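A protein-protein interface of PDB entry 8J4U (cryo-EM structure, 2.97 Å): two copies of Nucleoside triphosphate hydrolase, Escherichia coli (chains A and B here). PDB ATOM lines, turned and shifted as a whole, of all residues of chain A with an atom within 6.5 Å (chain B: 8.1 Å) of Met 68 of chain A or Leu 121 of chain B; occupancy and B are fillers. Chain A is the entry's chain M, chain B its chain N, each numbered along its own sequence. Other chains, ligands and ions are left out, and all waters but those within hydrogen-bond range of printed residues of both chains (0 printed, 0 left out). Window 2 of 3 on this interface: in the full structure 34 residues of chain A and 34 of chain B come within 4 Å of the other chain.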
ATOM      1  N   LEU A  27     -26.325  -5.072   0.181  1.00  0.00           N
ATOM      2  CA  LEU A  27     -27.748  -4.947   0.455  1.00  0.00           C
ATOM      3  C   LEU A  27     -28.136  -3.482   0.630  1.00  0.00           C
ATOM      4  O   LEU A  27     -27.294  -2.580   0.621  1.00  0.00           O
ATOM      5  CB  LEU A  27     -28.112  -5.758   1.699  1.00  0.00           C
ATOM      6  CG  LEU A  27     -28.674  -7.162   1.475  1.00  0.00           C
ATOM      7  CD1 LEU A  27     -27.656  -8.073   0.826  1.00  0.00           C
ATOM      8  CD2 LEU A  27     -29.128  -7.745   2.787  1.00  0.00           C
ATOM      9  N   GLN A  32     -33.762  -5.878   7.406  1.00  0.00           N
ATOM     10  CA  GLN A  32     -33.165  -6.729   8.429  1.00  0.00           C
ATOM     11  C   GLN A  32     -33.733  -8.141   8.450  1.00  0.00           C
ATOM     12  O   GLN A  32     -32.970  -9.111   8.402  1.00  0.00           O
ATOM     13  CB  GLN A  32     -33.338  -6.088   9.817  1.00  0.00           C
ATOM     14  CG  GLN A  32     -33.134  -4.581   9.864  1.00  0.00           C
ATOM     15  CD  GLN A  32     -31.740  -4.157   9.454  1.00  0.00           C
ATOM     16  OE1 GLN A  32     -30.899  -4.987   9.112  1.00  0.00           O
ATOM     17  NE2 GLN A  32     -31.483  -2.855   9.498  1.00  0.00           N
ATOM     18  N   THR A  46     -32.434 -14.523   2.912  1.00  0.00           N
ATOM     19  CA  THR A  46     -31.111 -14.267   3.478  1.00  0.00           C
ATOM     20  C   THR A  46     -30.348 -15.493   3.960  1.00  0.00           C
ATOM     21  O   THR A  46     -29.124 -15.410   4.092  1.00  0.00           O
ATOM     22  CB  THR A  46     -31.207 -13.295   4.663  1.00  0.00           C
ATOM     23  OG1 THR A  46     -32.101 -13.819   5.652  1.00  0.00           O
ATOM     24  CG2 THR A  46     -31.674 -11.928   4.215  1.00  0.00           C
ATOM     25  N   GLN A  47     -31.005 -16.607   4.226  1.00  0.00           N
ATOM     26  CA  GLN A  47     -30.287 -17.689   4.881  1.00  0.00           C
ATOM     27  C   GLN A  47     -29.556 -18.566   3.874  1.00  0.00           C
ATOM     28  O   GLN A  47     -29.943 -18.649   2.705  1.00  0.00           O
ATOM     29  CB  GLN A  47     -31.252 -18.540   5.696  1.00  0.00           C
ATOM     30  CG  GLN A  47     -32.150 -17.742   6.618  1.00  0.00           C
ATOM     31  CD  GLN A  47     -31.369 -16.897   7.602  1.00  0.00           C
ATOM     32  OE1 GLN A  47     -30.719 -15.922   7.224  1.00  0.00           O
ATOM     33  NE2 GLN A  47     -31.424 -17.270   8.871  1.00  0.00           N
ATOM     34  N   PRO A  48     -28.486 -19.240   4.302  1.00  0.00           N
ATOM     35  CA  PRO A  48     -27.828 -20.207   3.417  1.00  0.00           C
ATOM     36  C   PRO A  48     -28.754 -21.357   3.069  1.00  0.00           C
ATOM     37  O   PRO A  48     -29.565 -21.798   3.887  1.00  0.00           O
ATOM     38  CB  PRO A  48     -26.628 -20.683   4.242  1.00  0.00           C
ATOM     39  CG  PRO A  48     -26.363 -19.585   5.182  1.00  0.00           C
ATOM     40  CD  PRO A  48     -27.701 -19.015   5.527  1.00  0.00           C
ATOM     41  N   VAL A  65     -27.457 -19.314  -2.140  1.00  0.00           N
ATOM     42  CA  VAL A  65     -26.701 -18.556  -1.148  1.00  0.00           C
ATOM     43  C   VAL A  65     -25.760 -19.487  -0.399  1.00  0.00           C
ATOM     44  O   VAL A  65     -26.090 -20.650  -0.139  1.00  0.00           O
ATOM     45  CB  VAL A  65     -27.655 -17.841  -0.175  1.00  0.00           C
ATOM     46  CG1 VAL A  65     -26.875 -16.983   0.793  1.00  0.00           C
ATOM     47  CG2 VAL A  65     -28.659 -17.001  -0.925  1.00  0.00           C
ATOM     48  N   THR A  66     -24.580 -18.976  -0.042  1.00  0.00           N
ATOM     49  CA  THR A  66     -23.618 -19.735   0.748  1.00  0.00           C
ATOM     50  C   THR A  66     -23.258 -19.051   2.057  1.00  0.00           C
ATOM     51  O   THR A  66     -23.275 -19.698   3.111  1.00  0.00           O
ATOM     52  CB  THR A  66     -22.341 -19.990  -0.064  1.00  0.00           C
ATOM     53  OG1 THR A  66     -21.940 -18.786  -0.728  1.00  0.00           O
ATOM     54  CG2 THR A  66     -22.571 -21.084  -1.083  1.00  0.00           C
ATOM     55  N   ASP A  67     -22.932 -17.761   2.026  1.00  0.00           N
ATOM     56  CA  ASP A  67     -22.418 -17.056   3.190  1.00  0.00           C
ATOM     57  C   ASP A  67     -23.268 -15.824   3.480  1.00  0.00           C
ATOM     58  O   ASP A  67     -24.186 -15.476   2.733  1.00  0.00           O
ATOM     59  CB  ASP A  67     -20.952 -16.656   2.987  1.00  0.00           C
ATOM     60  CG  ASP A  67     -20.038 -17.851   2.834  1.00  0.00           C
ATOM     61  OD1 ASP A  67     -20.548 -18.990   2.798  1.00  0.00           O
ATOM     62  OD2 ASP A  67     -18.808 -17.653   2.750  1.00  0.00           O
ATOM     63  N   MET A  68     -22.941 -15.170   4.592  1.00  0.00           N
ATOM     64  CA  MET A  68     -23.665 -14.011   5.095  1.00  0.00           C
ATOM     65  C   MET A  68     -22.810 -13.349   6.168  1.00  0.00           C
ATOM     66  O   MET A  68     -22.415 -14.018   7.127  1.00  0.00           O
ATOM     67  CB  MET A  68     -25.019 -14.447   5.659  1.00  0.00           C
ATOM     68  CG  MET A  68     -25.964 -13.329   6.047  1.00  0.00           C
ATOM     69  SD  MET A  68     -26.673 -12.446   4.653  1.00  0.00           S
ATOM     70  CE  MET A  68     -27.371 -11.029   5.486  1.00  0.00           C
ATOM     71  N   ALA A  69     -22.505 -12.059   6.044  1.00  0.00           N
ATOM     72  CA  ALA A  69     -21.580 -11.469   7.004  1.00  0.00           C
ATOM     73  C   ALA A  69     -21.694  -9.952   7.006  1.00  0.00           C
ATOM     74  O   ALA A  69     -22.417  -9.357   6.206  1.00  0.00           O
ATOM     75  CB  ALA A  69     -20.143 -11.892   6.707  1.00  0.00           C
ATOM     76  N   PHE A  70     -20.976  -9.337   7.947  1.00  0.00           N
ATOM     77  CA  PHE A  70     -20.816  -7.889   8.004  1.00  0.00           C
ATOM     78  C   PHE A  70     -19.603  -7.492   7.174  1.00  0.00           C
ATOM     79  O   PHE A  70     -18.491  -7.965   7.433  1.00  0.00           O
ATOM     80  CB  PHE A  70     -20.631  -7.400   9.440  1.00  0.00           C
ATOM     81  CG  PHE A  70     -21.901  -7.311  10.235  1.00  0.00           C
ATOM     82  CD1 PHE A  70     -22.929  -6.476   9.839  1.00  0.00           C
ATOM     83  CD2 PHE A  70     -22.047  -8.026  11.409  1.00  0.00           C
ATOM     84  CE1 PHE A  70     -24.088  -6.385  10.579  1.00  0.00           C
ATOM     85  CE2 PHE A  70     -23.204  -7.935  12.151  1.00  0.00           C
ATOM     86  CZ  PHE A  70     -24.223  -7.113  11.735  1.00  0.00           C
ATOM     87  N   ARG A  92     -23.817  -5.070   5.328  1.00  0.00           N
ATOM     88  CA  ARG A  92     -23.936  -6.511   5.162  1.00  0.00           C
ATOM     89  C   ARG A  92     -23.429  -6.949   3.791  1.00  0.00           C
ATOM     90  O   ARG A  92     -23.278  -6.146   2.869  1.00  0.00           O
ATOM     91  CB  ARG A  92     -25.388  -6.943   5.345  1.00  0.00           C
ATOM     92  CG  ARG A  92     -26.077  -6.261   6.502  1.00  0.00           C
ATOM     93  CD  ARG A  92     -27.465  -6.810   6.744  1.00  0.00           C
ATOM     94  NE  ARG A  92     -27.886  -6.601   8.126  1.00  0.00           N
ATOM     95  CZ  ARG A  92     -28.723  -7.393   8.791  1.00  0.00           C
ATOM     96  NH1 ARG A  92     -29.256  -8.458   8.207  1.00  0.00           N
ATOM     97  NH2 ARG A  92     -29.034  -7.111  10.048  1.00  0.00           N
ATOM     98  N   GLN A  93     -23.174  -8.251   3.664  1.00  0.00           N
ATOM     99  CA  GLN A  93     -22.624  -8.796   2.432  1.00  0.00           C
ATOM    100  C   GLN A  93     -22.985 -10.271   2.316  1.00  0.00           C
ATOM    101  O   GLN A  93     -23.101 -10.981   3.323  1.00  0.00           O
ATOM    102  CB  GLN A  93     -21.106  -8.608   2.380  1.00  0.00           C
ATOM    103  CG  GLN A  93     -20.502  -8.851   1.014  1.00  0.00           C
ATOM    104  CD  GLN A  93     -19.015  -8.580   0.976  1.00  0.00           C
ATOM    105  OE1 GLN A  93     -18.202  -9.481   1.180  1.00  0.00           O
ATOM    106  NE2 GLN A  93     -18.649  -7.332   0.712  1.00  0.00           N
ATOM    107  N   ILE A  94     -23.128 -10.721   1.062  1.00  0.00           N
ATOM    108  CA  ILE A  94     -23.618 -12.055   0.731  1.00  0.00           C
ATOM    109  C   ILE A  94     -22.767 -12.653  -0.383  1.00  0.00           C
ATOM    110  O   ILE A  94     -22.195 -11.942  -1.212  1.00  0.00           O
ATOM    111  CB  ILE A  94     -25.102 -12.019   0.299  1.00  0.00           C
ATOM    112  CG1 ILE A  94     -25.993 -11.731   1.499  1.00  0.00           C
ATOM    113  CG2 ILE A  94     -25.519 -13.325  -0.350  1.00  0.00           C
ATOM    114  CD1 ILE A  94     -27.448 -11.607   1.155  1.00  0.00           C
ATOM    115  N   ILE A  95     -22.729 -13.989  -0.415  1.00  0.00           N
ATOM    116  CA  ILE A  95     -21.996 -14.753  -1.419  1.00  0.00           C
ATOM    117  C   ILE A  95     -22.927 -15.812  -1.997  1.00  0.00           C
ATOM    118  O   ILE A  95     -23.693 -16.449  -1.264  1.00  0.00           O
ATOM    119  CB  ILE A  95     -20.734 -15.414  -0.827  1.00  0.00           C
ATOM    120  CG1 ILE A  95     -19.914 -14.404  -0.018  1.00  0.00           C
ATOM    121  CG2 ILE A  95     -19.886 -16.011  -1.928  1.00  0.00           C
ATOM    122  CD1 ILE A  95     -19.261 -13.338  -0.841  1.00  0.00           C
ATOM    123  N   TYR B  14     -23.039 -11.535  20.509  1.00  0.00           N
ATOM    124  CA  TYR B  14     -23.851 -11.292  19.325  1.00  0.00           C
ATOM    125  C   TYR B  14     -23.243 -11.984  18.112  1.00  0.00           C
ATOM    126  O   TYR B  14     -22.021 -12.114  18.001  1.00  0.00           O
ATOM    127  CB  TYR B  14     -24.026  -9.788  19.066  1.00  0.00           C
ATOM    128  CG  TYR B  14     -22.748  -9.003  18.877  1.00  0.00           C
ATOM    129  CD1 TYR B  14     -22.036  -8.525  19.968  1.00  0.00           C
ATOM    130  CD2 TYR B  14     -22.272  -8.711  17.609  1.00  0.00           C
ATOM    131  CE1 TYR B  14     -20.879  -7.804  19.801  1.00  0.00           C
ATOM    132  CE2 TYR B  14     -21.117  -7.986  17.433  1.00  0.00           C
ATOM    133  CZ  TYR B  14     -20.424  -7.535  18.532  1.00  0.00           C
ATOM    134  OH  TYR B  14     -19.269  -6.812  18.364  1.00  0.00           O
ATOM    135  N   VAL B  15     -24.121 -12.444  17.217  1.00  0.00           N
ATOM    136  CA  VAL B  15     -23.710 -13.148  16.008  1.00  0.00           C
ATOM    137  C   VAL B  15     -23.122 -12.172  15.001  1.00  0.00           C
ATOM    138  O   VAL B  15     -23.646 -11.069  14.799  1.00  0.00           O
ATOM    139  CB  VAL B  15     -24.909 -13.895  15.401  1.00  0.00           C
ATOM    140  CG1 VAL B  15     -24.502 -14.627  14.153  1.00  0.00           C
ATOM    141  CG2 VAL B  15     -25.518 -14.856  16.399  1.00  0.00           C
ATOM    142  N   VAL B  16     -22.033 -12.581  14.346  1.00  0.00           N
ATOM    143  CA  VAL B  16     -21.398 -11.764  13.319  1.00  0.00           C
ATOM    144  C   VAL B  16     -21.070 -12.540  12.052  1.00  0.00           C
ATOM    145  O   VAL B  16     -20.533 -11.956  11.111  1.00  0.00           O
ATOM    146  CB  VAL B  16     -20.129 -11.068  13.853  1.00  0.00           C
ATOM    147  CG1 VAL B  16     -20.465 -10.200  15.032  1.00  0.00           C
ATOM    148  CG2 VAL B  16     -19.081 -12.075  14.229  1.00  0.00           C
ATOM    149  N   GLY B  17     -21.367 -13.834  11.986  1.00  0.00           N
ATOM    150  CA  GLY B  17     -21.064 -14.580  10.781  1.00  0.00           C
ATOM    151  C   GLY B  17     -21.696 -15.949  10.678  1.00  0.00           C
ATOM    152  O   GLY B  17     -21.821 -16.670  11.671  1.00  0.00           O
ATOM    153  N   LEU B  18     -22.100 -16.313   9.462  1.00  0.00           N
ATOM    154  CA  LEU B  18     -22.565 -17.656   9.139  1.00  0.00           C
ATOM    155  C   LEU B  18     -21.819 -18.138   7.904  1.00  0.00           C
ATOM    156  O   LEU B  18     -21.875 -17.492   6.854  1.00  0.00           O
ATOM    157  CB  LEU B  18     -24.073 -17.690   8.884  1.00  0.00           C
ATOM    158  CG  LEU B  18     -24.999 -16.976   9.865  1.00  0.00           C
ATOM    159  CD1 LEU B  18     -26.349 -16.748   9.235  1.00  0.00           C
ATOM    160  CD2 LEU B  18     -25.152 -17.774  11.135  1.00  0.00           C
ATOM    161  N   GLU B  19     -21.125 -19.267   8.031  1.00  0.00           N
ATOM    162  CA  GLU B  19     -20.389 -19.881   6.926  1.00  0.00           C
ATOM    163  C   GLU B  19     -20.811 -21.344   6.856  1.00  0.00           C
ATOM    164  O   GLU B  19     -20.165 -22.216   7.442  1.00  0.00           O
ATOM    165  CB  GLU B  19     -18.884 -19.734   7.108  1.00  0.00           C
ATOM    166  CG  GLU B  19     -18.437 -18.325   7.458  1.00  0.00           C
ATOM    167  CD  GLU B  19     -18.022 -18.173   8.911  1.00  0.00           C
ATOM    168  OE1 GLU B  19     -18.416 -19.015   9.744  1.00  0.00           O
ATOM    169  OE2 GLU B  19     -17.299 -17.203   9.220  1.00  0.00           O
ATOM    170  N   GLY B  20     -21.892 -21.608   6.131  1.00  0.00           N
ATOM    171  CA  GLY B  20     -22.419 -22.950   6.026  1.00  0.00           C
ATOM    172  C   GLY B  20     -23.146 -23.384   7.279  1.00  0.00           C
ATOM    173  O   GLY B  20     -24.189 -22.822   7.627  1.00  0.00           O
ATOM    174  N   ARG B  22     -21.592 -23.360  10.292  1.00  0.00           N
ATOM    175  CA  ARG B  22     -20.953 -22.716  11.426  1.00  0.00           C
ATOM    176  C   ARG B  22     -21.682 -21.444  11.841  1.00  0.00           C
ATOM    177  O   ARG B  22     -22.431 -20.837  11.072  1.00  0.00           O
ATOM    178  CB  ARG B  22     -19.505 -22.372  11.101  1.00  0.00           C
ATOM    179  CG  ARG B  22     -18.627 -23.564  10.837  1.00  0.00           C
ATOM    180  CD  ARG B  22     -17.209 -23.126  10.553  1.00  0.00           C
ATOM    181  NE  ARG B  22     -16.236 -24.124  10.978  1.00  0.00           N
ATOM    182  CZ  ARG B  22     -14.934 -23.891  11.102  1.00  0.00           C
ATOM    183  NH1 ARG B  22     -14.442 -22.692  10.830  1.00  0.00           N
ATOM    184  NH2 ARG B  22     -14.123 -24.858  11.502  1.00  0.00           N
ATOM    185  N   ARG B  24     -20.710 -17.794  14.261  1.00  0.00           N
ATOM    186  CA  ARG B  24     -19.605 -17.027  14.818  1.00  0.00           C
ATOM    187  C   ARG B  24     -20.139 -15.934  15.731  1.00  0.00           C
ATOM    188  O   ARG B  24     -21.031 -15.170  15.344  1.00  0.00           O
ATOM    189  CB  ARG B  24     -18.741 -16.425  13.712  1.00  0.00           C
ATOM    190  CG  ARG B  24     -17.343 -16.092  14.164  1.00  0.00           C
ATOM    191  CD  ARG B  24     -16.644 -15.148  13.214  1.00  0.00           C
ATOM    192  NE  ARG B  24     -16.210 -15.828  12.001  1.00  0.00           N
ATOM    193  CZ  ARG B  24     -15.055 -16.474  11.871  1.00  0.00           C
ATOM    194  NH1 ARG B  24     -14.199 -16.544  12.879  1.00  0.00           N
ATOM    195  NH2 ARG B  24     -14.756 -17.060  10.723  1.00  0.00           N
ATOM    196  N   LEU B 118     -31.024 -21.892  11.195  1.00  0.00           N
ATOM    197  CA  LEU B 118     -29.964 -21.068  11.751  1.00  0.00           C
ATOM    198  C   LEU B 118     -30.547 -19.757  12.247  1.00  0.00           C
ATOM    199  O   LEU B 118     -31.675 -19.396  11.895  1.00  0.00           O
ATOM    200  CB  LEU B 118     -28.878 -20.787  10.705  1.00  0.00           C
ATOM    201  CG  LEU B 118     -28.101 -21.983  10.160  1.00  0.00           C
ATOM    202  CD1 LEU B 118     -27.012 -21.521   9.224  1.00  0.00           C
ATOM    203  CD2 LEU B 118     -27.504 -22.796  11.282  1.00  0.00           C
ATOM    204  N   PRO B 119     -29.806 -19.022  13.083  1.00  0.00           N
ATOM    205  CA  PRO B 119     -30.280 -17.706  13.523  1.00  0.00           C
ATOM    206  C   PRO B 119     -29.904 -16.590  12.561  1.00  0.00           C
ATOM    207  O   PRO B 119     -29.309 -16.840  11.509  1.00  0.00           O
ATOM    208  CB  PRO B 119     -29.592 -17.533  14.879  1.00  0.00           C
ATOM    209  CG  PRO B 119     -28.346 -18.290  14.741  1.00  0.00           C
ATOM    210  CD  PRO B 119     -28.645 -19.466  13.870  1.00  0.00           C
ATOM    211  N   ALA B 120     -30.244 -15.356  12.918  1.00  0.00           N
ATOM    212  CA  ALA B 120     -30.043 -14.198  12.062  1.00  0.00           C
ATOM    213  C   ALA B 120     -28.993 -13.267  12.652  1.00  0.00           C
ATOM    214  O   ALA B 120     -28.877 -13.139  13.875  1.00  0.00           O
ATOM    215  CB  ALA B 120     -31.352 -13.436  11.866  1.00  0.00           C
ATOM    216  N   LEU B 121     -28.231 -12.620  11.771  1.00  0.00           N
ATOM    217  CA  LEU B 121     -27.226 -11.648  12.182  1.00  0.00           C
ATOM    218  C   LEU B 121     -27.788 -10.664  13.196  1.00  0.00           C
ATOM    219  O   LEU B 121     -28.933 -10.219  13.090  1.00  0.00           O
ATOM    220  CB  LEU B 121     -26.699 -10.890  10.967  1.00  0.00           C
ATOM    221  CG  LEU B 121     -25.579 -11.561  10.179  1.00  0.00           C
ATOM    222  CD1 LEU B 121     -26.071 -12.791   9.480  1.00  0.00           C
ATOM    223  CD2 LEU B 121     -25.017 -10.588   9.186  1.00  0.00           C
ATOM    224  N   GLY B 122     -26.962 -10.322  14.181  1.00  0.00           N
ATOM    225  CA  GLY B 122     -27.350  -9.417  15.235  1.00  0.00           C
ATOM    226  C   GLY B 122     -28.059 -10.064  16.401  1.00  0.00           C
ATOM    227  O   GLY B 122     -28.199  -9.424  17.450  1.00  0.00           O
ATOM    228  N   SER B 123     -28.507 -11.307  16.255  1.00  0.00           N
ATOM    229  CA  SER B 123     -29.187 -11.985  17.343  1.00  0.00           C
ATOM    230  C   SER B 123     -28.285 -12.061  18.570  1.00  0.00           C
ATOM    231  O   SER B 123     -27.062 -11.943  18.487  1.00  0.00           O
ATOM    232  CB  SER B 123     -29.617 -13.383  16.909  1.00  0.00           C
ATOM    233  OG  SER B 123     -30.558 -13.321  15.858  1.00  0.00           O
ATOM    234  N   SER B 124     -28.913 -12.259  19.724  1.00  0.00           N
ATOM    235  CA  SER B 124     -28.229 -12.272  21.006  1.00  0.00           C
ATOM    236  C   SER B 124     -28.180 -13.686  21.565  1.00  0.00           C
ATOM    237  O   SER B 124     -29.162 -14.430  21.490  1.00  0.00           O
ATOM    238  CB  SER B 124     -28.924 -11.341  21.996  1.00  0.00           C
ATOM    239  OG  SER B 124     -30.291 -11.676  22.134  1.00  0.00           O
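Of the 15 printed residues of chain A, 4 touch a printed residue of chain B.
Hydrophobic or aromatic side chains of chain A that line the printed part of chain B: Met 68.
No position is printed for both chains.
N of Thr 66 of chain A lies within hydrogen-bond range of O of Ile 95 of chain A.
The side-chain amide oxygen (OE1) of Gln 47 of chain A sits at hydrogen-bond distance from the side-chain hydroxyl (OG1) of Thr 46 of chain A (3.0 Å).
O of Gly 17 of chain B is in hydrogen-bond range of N of Arg 24 of chain B, at 3.0 Å.
Gln 47 of chain A touches Leu 118 of chain B (NE2 to O, 3.7 Å).
Thr 66 of chain A touches Gly 20 of chain B (O to N, 3.8 Å).
Leu 18 of chain B touches Asp 67 of chain A (O to CA, 3.7 Å).
Gly 17 of chain B touches Met 68 of chain A (CA to O, 3.9 Å).
Met 68 of chain A touches Leu 121 of chain B.
N of Leu 18 of chain B is in hydrogen-bond range of O of Met 68 of chain A (3.3 Å).
NE2 of Gln 47 of chain A is in hydrogen-bond range of O of Pro 119 of chain B (3.4 Å).
Of the printed residues of chain B, Gln 47 of chain A touches Leu 118 and Pro 119.
Of the printed residues of chain B, Thr 66 of chain A touches Gly 20.
Printed residues of chain B within 4 Å of Asp 67 of chain A: Leu 18 (3.7 Å).
Met 68 of chain A touches just these residues of chain B: Gly 17, Leu 18 and Leu 121.
No residue of chain B comes within 4 Å of Ala 69 of chain A.
Ser 123 of chain B touches none of the printed residues of chain A.
The nearest residue of chain A that does not touch Leu 121 of chain B is Ala 69 of chain A (4.02 Å).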
